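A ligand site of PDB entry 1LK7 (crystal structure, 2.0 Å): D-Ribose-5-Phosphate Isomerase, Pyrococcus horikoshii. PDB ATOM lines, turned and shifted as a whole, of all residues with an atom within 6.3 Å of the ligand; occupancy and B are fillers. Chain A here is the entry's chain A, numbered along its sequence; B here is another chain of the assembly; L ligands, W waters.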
ATOM      1  N   LYS A   7      12.919  -3.980  -5.038  1.00  0.00           N
ATOM      2  CA  LYS A   7      12.854  -2.520  -4.849  1.00  0.00           C
ATOM      3  C   LYS A   7      11.493  -1.981  -5.276  1.00  0.00           C
ATOM      4  O   LYS A   7      10.913  -1.135  -4.597  1.00  0.00           O
ATOM      5  CB  LYS A   7      13.917  -1.834  -5.709  1.00  0.00           C
ATOM      6  CG  LYS A   7      15.341  -1.944  -5.196  1.00  0.00           C
ATOM      7  CD  LYS A   7      16.307  -1.376  -6.231  1.00  0.00           C
ATOM      8  CE  LYS A   7      17.740  -1.333  -5.727  1.00  0.00           C
ATOM      9  NZ  LYS A   7      18.701  -0.892  -6.767  1.00  0.00           N
ATOM     10  N   GLY A  27      12.529  11.295  -2.095  1.00  0.00           N
ATOM     11  CA  GLY A  27      13.869  10.818  -1.838  1.00  0.00           C
ATOM     12  C   GLY A  27      14.736  10.588  -3.039  1.00  0.00           C
ATOM     13  O   GLY A  27      14.326  10.703  -4.167  1.00  0.00           O
ATOM     14  N   THR A  28      15.968  10.186  -2.764  1.00  0.00           N
ATOM     15  CA  THR A  28      16.966  10.032  -3.795  1.00  0.00           C
ATOM     16  C   THR A  28      17.405   8.592  -3.988  1.00  0.00           C
ATOM     17  O   THR A  28      17.497   7.838  -3.031  1.00  0.00           O
ATOM     18  CB  THR A  28      18.156  10.895  -3.349  1.00  0.00           C
ATOM     19  OG1 THR A  28      17.763  12.274  -3.384  1.00  0.00           O
ATOM     20  CG2 THR A  28      19.297  10.782  -4.317  1.00  0.00           C
ATOM     21  N   GLY A  29      17.657   8.198  -5.227  1.00  0.00           N
ATOM     22  CA  GLY A  29      18.218   6.895  -5.490  1.00  0.00           C
ATOM     23  C   GLY A  29      17.276   5.973  -6.258  1.00  0.00           C
ATOM     24  O   GLY A  29      16.092   6.294  -6.457  1.00  0.00           O
ATOM     25  N   SER A  30      17.793   4.794  -6.616  1.00  0.00           N
ATOM     26  CA  SER A  30      17.100   3.825  -7.477  1.00  0.00           C
ATOM     27  C   SER A  30      15.794   3.229  -6.921  1.00  0.00           C
ATOM     28  O   SER A  30      14.856   3.012  -7.688  1.00  0.00           O
ATOM     29  CB  SER A  30      18.066   2.700  -7.869  1.00  0.00           C
ATOM     30  OG  SER A  30      18.452   1.921  -6.742  1.00  0.00           O
ATOM     31  N   THR A  31      15.721   2.955  -5.634  1.00  0.00           N
ATOM     32  CA  THR A  31      14.513   2.378  -5.033  1.00  0.00           C
ATOM     33  C   THR A  31      13.417   3.460  -5.021  1.00  0.00           C
ATOM     34  O   THR A  31      12.286   3.266  -5.520  1.00  0.00           O
ATOM     35  CB  THR A  31      14.779   1.906  -3.580  1.00  0.00           C
ATOM     36  OG1 THR A  31      15.987   1.122  -3.484  1.00  0.00           O
ATOM     37  CG2 THR A  31      13.692   0.938  -3.082  1.00  0.00           C
ATOM     38  N   THR A  32      13.744   4.600  -4.407  1.00  0.00           N
ATOM     39  CA  THR A  32      12.816   5.693  -4.430  1.00  0.00           C
ATOM     40  C   THR A  32      12.452   6.129  -5.857  1.00  0.00           C
ATOM     41  O   THR A  32      11.335   6.545  -6.105  1.00  0.00           O
ATOM     42  CB  THR A  32      13.350   6.856  -3.578  1.00  0.00           C
ATOM     43  OG1 THR A  32      13.428   6.433  -2.205  1.00  0.00           O
ATOM     44  CG2 THR A  32      12.363   8.010  -3.548  1.00  0.00           C
ATOM     45  N   ALA A  33      13.364   6.005  -6.817  1.00  0.00           N
ATOM     46  CA  ALA A  33      12.997   6.395  -8.194  1.00  0.00           C
ATOM     47  C   ALA A  33      11.756   5.633  -8.685  1.00  0.00           C
ATOM     48  O   ALA A  33      10.936   6.156  -9.438  1.00  0.00           O
ATOM     49  CB  ALA A  33      14.172   6.173  -9.149  1.00  0.00           C
ATOM     50  N   ASP A  85      12.117   7.737   1.179  1.00  0.00           N
ATOM     51  CA  ASP A  85      13.476   7.733   0.703  1.00  0.00           C
ATOM     52  C   ASP A  85      14.111   6.364   0.882  1.00  0.00           C
ATOM     53  O   ASP A  85      13.523   5.498   1.528  1.00  0.00           O
ATOM     54  CB  ASP A  85      14.257   8.803   1.488  1.00  0.00           C
ATOM     55  CG  ASP A  85      15.508   9.256   0.780  1.00  0.00           C
ATOM     56  OD1 ASP A  85      16.058  10.335   1.136  1.00  0.00           O
ATOM     57  OD2 ASP A  85      15.994   8.636  -0.172  1.00  0.00           O
ATOM     58  N   GLY A  86      15.280   6.149   0.289  1.00  0.00           N
ATOM     59  CA  GLY A  86      16.032   4.940   0.509  1.00  0.00           C
ATOM     60  C   GLY A  86      17.025   5.031   1.656  1.00  0.00           C
ATOM     61  O   GLY A  86      16.987   5.973   2.457  1.00  0.00           O
ATOM     62  N   ALA A  87      17.918   4.052   1.702  1.00  0.00           N
ATOM     63  CA  ALA A  87      18.948   3.947   2.715  1.00  0.00           C
ATOM     64  C   ALA A  87      20.010   2.961   2.260  1.00  0.00           C
ATOM     65  O   ALA A  87      19.724   2.066   1.462  1.00  0.00           O
ATOM     66  CB  ALA A  87      18.371   3.494   4.037  1.00  0.00           C
ATOM     67  N   ASP A  88      21.234   3.132   2.755  1.00  0.00           N
ATOM     68  CA  ASP A  88      22.324   2.224   2.434  1.00  0.00           C
ATOM     69  C   ASP A  88      22.387   1.077   3.466  1.00  0.00           C
ATOM     70  O   ASP A  88      22.867  -0.019   3.153  1.00  0.00           O
ATOM     71  CB  ASP A  88      23.663   2.941   2.464  1.00  0.00           C
ATOM     72  CG  ASP A  88      23.676   4.185   1.616  1.00  0.00           C
ATOM     73  OD1 ASP A  88      23.233   4.128   0.452  1.00  0.00           O
ATOM     74  OD2 ASP A  88      24.119   5.272   2.052  1.00  0.00           O
ATOM     75  N   GLU A  89      21.955   1.362   4.704  1.00  0.00           N
ATOM     76  CA  GLU A  89      21.794   0.360   5.727  1.00  0.00           C
ATOM     77  C   GLU A  89      20.561   0.627   6.606  1.00  0.00           C
ATOM     78  O   GLU A  89      20.175   1.782   6.870  1.00  0.00           O
ATOM     79  CB  GLU A  89      23.025   0.289   6.660  1.00  0.00           C
ATOM     80  CG  GLU A  89      24.248  -0.446   6.089  1.00  0.00           C
ATOM     81  CD  GLU A  89      25.399  -0.577   7.089  1.00  0.00           C
ATOM     82  OE1 GLU A  89      25.310  -0.133   8.243  1.00  0.00           O
ATOM     83  OE2 GLU A  89      26.431  -1.143   6.711  1.00  0.00           O
ATOM     84  N   ILE A  97      21.925   4.287   7.703  1.00  0.00           N
ATOM     85  CA  ILE A  97      22.995   5.030   7.076  1.00  0.00           C
ATOM     86  C   ILE A  97      22.458   5.430   5.720  1.00  0.00           C
ATOM     87  O   ILE A  97      21.942   4.607   4.976  1.00  0.00           O
ATOM     88  CB  ILE A  97      24.269   4.227   6.832  1.00  0.00           C
ATOM     89  CG1 ILE A  97      24.951   3.836   8.125  1.00  0.00           C
ATOM     90  CG2 ILE A  97      25.248   5.075   6.016  1.00  0.00           C
ATOM     91  CD1 ILE A  97      26.237   3.099   7.881  1.00  0.00           C
ATOM     92  N   LYS A  98      22.630   6.694   5.391  1.00  0.00           N
ATOM     93  CA  LYS A  98      22.261   7.187   4.067  1.00  0.00           C
ATOM     94  C   LYS A  98      23.447   8.007   3.524  1.00  0.00           C
ATOM     95  O   LYS A  98      24.384   8.308   4.269  1.00  0.00           O
ATOM     96  CB  LYS A  98      21.013   8.054   4.150  1.00  0.00           C
ATOM     97  CG  LYS A  98      19.685   7.290   4.410  1.00  0.00           C
ATOM     98  CD  LYS A  98      18.427   8.188   4.542  1.00  0.00           C
ATOM     99  CE  LYS A  98      18.248   9.174   3.402  1.00  0.00           C
ATOM    100  NZ  LYS A  98      18.232   8.504   2.100  1.00  0.00           N
ATOM    101  N   GLY A  99      23.380   8.399   2.259  1.00  0.00           N
ATOM    102  CA  GLY A  99      24.417   9.234   1.667  1.00  0.00           C
ATOM    103  C   GLY A  99      25.215   8.699   0.510  1.00  0.00           C
ATOM    104  O   GLY A  99      26.010   9.441  -0.091  1.00  0.00           O
ATOM    105  N   ARG A 100      24.996   7.450   0.110  1.00  0.00           N
ATOM    106  CA  ARG A 100      25.719   6.914  -1.047  1.00  0.00           C
ATOM    107  C   ARG A 100      25.521   7.891  -2.218  1.00  0.00           C
ATOM    108  O   ARG A 100      26.446   8.148  -3.008  1.00  0.00           O
ATOM    109  CB  ARG A 100      25.201   5.545  -1.483  1.00  0.00           C
ATOM    110  CG  ARG A 100      25.863   5.024  -2.761  1.00  0.00           C
ATOM    111  CD  ARG A 100      25.031   3.956  -3.542  1.00  0.00           C
ATOM    112  NE  ARG A 100      23.633   4.378  -3.670  1.00  0.00           N
ATOM    113  CZ  ARG A 100      23.184   5.305  -4.529  1.00  0.00           C
ATOM    114  NH1 ARG A 100      24.023   5.890  -5.385  1.00  0.00           N
ATOM    115  NH2 ARG A 100      21.898   5.628  -4.540  1.00  0.00           N
ATOM    116  N   GLY A 101      24.314   8.441  -2.296  1.00  0.00           N
ATOM    117  CA  GLY A 101      23.925   9.340  -3.396  1.00  0.00           C
ATOM    118  C   GLY A 101      24.408  10.789  -3.242  1.00  0.00           C
ATOM    119  O   GLY A 101      24.289  11.579  -4.176  1.00  0.00           O
ATOM    120  N   ALA A 102      24.884  11.100  -2.042  1.00  0.00           N
ATOM    121  CA  ALA A 102      25.517  12.382  -1.686  1.00  0.00           C
ATOM    122  C   ALA A 102      24.532  13.499  -1.459  1.00  0.00           C
ATOM    123  O   ALA A 102      24.916  14.665  -1.399  1.00  0.00           O
ATOM    124  CB  ALA A 102      26.575  12.779  -2.717  1.00  0.00           C
ATOM    125  N   ALA A 103      23.276  13.120  -1.234  1.00  0.00           N
ATOM    126  CA  ALA A 103      22.204  14.070  -1.048  1.00  0.00           C
ATOM    127  C   ALA A 103      21.752  14.149   0.405  1.00  0.00           C
ATOM    128  O   ALA A 103      20.654  14.653   0.712  1.00  0.00           O
ATOM    129  CB  ALA A 103      21.026  13.642  -1.927  1.00  0.00           C
ATOM    130  N   LEU A 104      22.601  13.687   1.319  1.00  0.00           N
ATOM    131  CA  LEU A 104      22.235  13.552   2.726  1.00  0.00           C
ATOM    132  C   LEU A 104      21.767  14.796   3.442  1.00  0.00           C
ATOM    133  O   LEU A 104      20.934  14.716   4.353  1.00  0.00           O
ATOM    134  CB  LEU A 104      23.351  12.854   3.533  1.00  0.00           C
ATOM    135  CG  LEU A 104      24.790  13.372   3.689  1.00  0.00           C
ATOM    136  CD1 LEU A 104      25.550  12.563   4.758  1.00  0.00           C
ATOM    137  CD2 LEU A 104      25.531  13.310   2.380  1.00  0.00           C
ATOM    138  N   GLU A 107      18.216  15.612   2.273  1.00  0.00           N
ATOM    139  CA  GLU A 107      17.401  14.501   2.744  1.00  0.00           C
ATOM    140  C   GLU A 107      17.049  14.662   4.210  1.00  0.00           C
ATOM    141  O   GLU A 107      15.892  14.482   4.596  1.00  0.00           O
ATOM    142  CB  GLU A 107      18.115  13.162   2.476  1.00  0.00           C
ATOM    143  CG  GLU A 107      18.118  12.749   1.013  1.00  0.00           C
ATOM    144  CD  GLU A 107      19.061  11.589   0.759  1.00  0.00           C
ATOM    145  OE1 GLU A 107      19.924  11.340   1.619  1.00  0.00           O
ATOM    146  OE2 GLU A 107      18.924  10.895  -0.248  1.00  0.00           O
ATOM    147  N   LEU A 120      12.390   2.934   2.118  1.00  0.00           N
ATOM    148  CA  LEU A 120      12.267   1.791   1.218  1.00  0.00           C
ATOM    149  C   LEU A 120      13.580   1.220   0.876  1.00  0.00           C
ATOM    150  O   LEU A 120      14.449   1.929   0.373  1.00  0.00           O
ATOM    151  CB  LEU A 120      11.719   2.239  -0.115  1.00  0.00           C
ATOM    152  CG  LEU A 120      10.573   3.205  -0.045  1.00  0.00           C
ATOM    153  CD1 LEU A 120      10.270   3.660  -1.472  1.00  0.00           C
ATOM    154  CD2 LEU A 120       9.384   2.552   0.609  1.00  0.00           C
ATOM    155  N   ASP A 122      15.640  -2.870  -0.335  1.00  0.00           N
ATOM    156  CA  ASP A 122      15.601  -4.308  -0.552  1.00  0.00           C
ATOM    157  C   ASP A 122      16.382  -5.028   0.558  1.00  0.00           C
ATOM    158  O   ASP A 122      17.027  -4.376   1.397  1.00  0.00           O
ATOM    159  CB  ASP A 122      16.192  -4.669  -1.901  1.00  0.00           C
ATOM    160  CG  ASP A 122      17.687  -4.440  -1.978  1.00  0.00           C
ATOM    161  OD1 ASP A 122      18.098  -3.439  -2.607  1.00  0.00           O
ATOM    162  OD2 ASP A 122      18.529  -5.204  -1.463  1.00  0.00           O
ATOM    163  N   ARG A 124      19.170  -6.591   0.921  1.00  0.00           N
ATOM    164  CA  ARG A 124      20.592  -6.349   1.139  1.00  0.00           C
ATOM    165  C   ARG A 124      20.857  -5.261   2.164  1.00  0.00           C
ATOM    166  O   ARG A 124      21.866  -5.321   2.855  1.00  0.00           O
ATOM    167  CB  ARG A 124      21.269  -5.978  -0.179  1.00  0.00           C
ATOM    168  CG  ARG A 124      21.228  -7.047  -1.253  1.00  0.00           C
ATOM    169  CD  ARG A 124      21.658  -6.515  -2.611  1.00  0.00           C
ATOM    170  NE  ARG A 124      20.964  -5.268  -2.889  1.00  0.00           N
ATOM    171  CZ  ARG A 124      21.386  -4.331  -3.737  1.00  0.00           C
ATOM    172  NH1 ARG A 124      22.501  -4.509  -4.432  1.00  0.00           N
ATOM    173  NH2 ARG A 124      20.662  -3.225  -3.894  1.00  0.00           N
ATOM    174  N   LYS A 125      19.954  -4.302   2.293  1.00  0.00           N
ATOM    175  CA  LYS A 125      20.192  -3.145   3.176  1.00  0.00           C
ATOM    176  C   LYS A 125      20.052  -3.463   4.655  1.00  0.00           C
ATOM    177  O   LYS A 125      20.571  -2.727   5.498  1.00  0.00           O
ATOM    178  CB  LYS A 125      19.277  -1.969   2.790  1.00  0.00           C
ATOM    179  CG  LYS A 125      19.243  -1.620   1.297  1.00  0.00           C
ATOM    180  CD  LYS A 125      20.612  -1.257   0.719  1.00  0.00           C
ATOM    181  CE  LYS A 125      20.496  -0.700  -0.712  1.00  0.00           C
ATOM    182  NZ  LYS A 125      19.467   0.360  -0.874  1.00  0.00           N
ATOM    183  N   ASP B 168      24.481  10.640  -6.990  1.00  0.00           N
ATOM    184  CA  ASP B 168      23.289  10.578  -7.842  1.00  0.00           C
ATOM    185  C   ASP B 168      23.073  11.974  -8.404  1.00  0.00           C
ATOM    186  O   ASP B 168      23.620  12.939  -7.870  1.00  0.00           O
ATOM    187  CB  ASP B 168      22.047  10.177  -7.049  1.00  0.00           C
ATOM    188  CG  ASP B 168      22.073   8.749  -6.554  1.00  0.00           C
ATOM    189  OD1 ASP B 168      22.768   7.884  -7.130  1.00  0.00           O
ATOM    190  OD2 ASP B 168      21.438   8.375  -5.540  1.00  0.00           O
HETATM  191  O1  LIG L   1      21.668   8.552  -1.112  1.00  0.00           O
HETATM  192  C1  LIG L   1      20.880   7.883  -0.439  1.00  0.00           C
HETATM  193  O2  LIG L   1      20.821   8.024   0.786  1.00  0.00           O
HETATM  194  C2  LIG L   1      20.000   6.862  -1.108  1.00  0.00           C
HETATM  195  O3  LIG L   1      18.646   6.942  -0.682  1.00  0.00           O
HETATM  196  C3  LIG L   1      20.568   5.498  -0.706  1.00  0.00           C
HETATM  197  O4  LIG L   1      20.483   5.423   0.698  1.00  0.00           O
HETATM  198  C4  LIG L   1      19.811   4.346  -1.330  1.00  0.00           C
HETATM  199  O5  LIG L   1      19.733   4.521  -2.757  1.00  0.00           O
HETATM  200  P1  LIG L   1      19.288   3.241  -3.604  1.00  0.00           P
HETATM  201  O6  LIG L   1      19.755   3.392  -5.025  1.00  0.00           O
HETATM  202  O7  LIG L   1      17.791   3.196  -3.442  1.00  0.00           O
HETATM  203  O8  LIG L   1      20.033   2.089  -2.991  1.00  0.00           O
HETATM  204  O   HOH W   1      17.171   2.049  -0.663  1.00  0.00           O
HETATM  205  O   HOH W   2      16.087   5.344  -2.979  1.00  0.00           O
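Gly 29 touches the ligand. Gly 86 touches the ligand (C to O3, 3.4 Å). Glu 107 touches the ligand (OE1 to O2, 3.5 Å). Of the 27 residues printed, 14 come within 4 Å of the ligand.
The side-chain hydroxyl (OG) of Ser 30 lies within hydrogen-bond range of the side-chain amino group (NZ) of Lys 7. The backbone NH (N) of Thr 28 is in hydrogen-bond range of the side-chain carboxylate (OD2) of Asp 85. The side-chain amino group (NZ) of Lys 125 lies within hydrogen-bond range of the backbone carbonyl oxygen (O) of Ala 87 (2.9 Å). The backbone carbonyl oxygen (O) of Gly 101 sits at hydrogen-bond distance from the backbone NH (N) of Asp 168 of chain B (3.0 Å). NZ of Lys 98 is in salt-bridge range of OE1 of Glu 107 (3.3 Å). N of Arg 100 is in hydrogen-bond range of OD2 of Asp 88. The guanidinium group of Arg 100 lies within salt-bridge range of the side-chain carboxylate of Asp 168 of chain B, 2.9 Å away. N of Asp 88 lies within hydrogen-bond range of O of Ile 97, 2.8 Å away.
Water W2 lies within hydrogen-bond range of an oxygen (O7) of the ligand (2.8 Å), the backbone NH (N) of Thr 32 (2.8 Å), the backbone carbonyl oxygen (O) of Thr 28 (2.9 Å) and the backbone NH (N) of Gly 86 (3.5 Å). Water W1 lies within hydrogen-bond range of NZ of Lys 125, O of Leu 120, O7 of the ligand, N of Ala 87 and OG1 of Thr 31.
O6 of the ligand is in hydrogen-bond range of N of Ser 30, at 2.9 Å. The side-chain hydroxyl (OG) of Ser 30 is in hydrogen-bond range of an oxygen (O6) of the ligand, at 2.6 Å. The backbone NH (N) of Thr 31 sits at hydrogen-bond distance from an oxygen (O7) of the ligand (3.0 Å). OG1 of Thr 31 is in hydrogen-bond range of O7 of the ligand, at 2.7 Å. An oxygen (O3) of the ligand is in hydrogen-bond range of the backbone carbonyl oxygen (O) of Thr 28 (2.8 Å). The side-chain amino group (NZ) of Lys 125 lies within salt-bridge range of an oxygen (O8) of the ligand, 2.8 Å away. The backbone NH (N) of Gly 101 lies within hydrogen-bond range of an oxygen (O1) of the ligand (2.9 Å). N of Ala 87 lies close to O4 of the ligand. The side-chain amino group (NZ) of Lys 98 sits at hydrogen-bond distance from an oxygen (O2) of the ligand, 2.9 Å away. N of Gly 99 is in hydrogen-bond range of O2 of the ligand. O6 of the ligand lies within salt-bridge range of NH2 of Arg 100 (3.1 Å). An oxygen (O4) of the ligand is in hydrogen-bond range of the backbone NH of Asp 88. The side-chain carboxylate (OD1) of Asp 88 is in hydrogen-bond range of an oxygen (O4) of the ligand (3.0 Å). An oxygen (O3) of the ligand lies within hydrogen-bond range of the side-chain carboxylate (OD2) of Asp 85 (3.2 Å).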
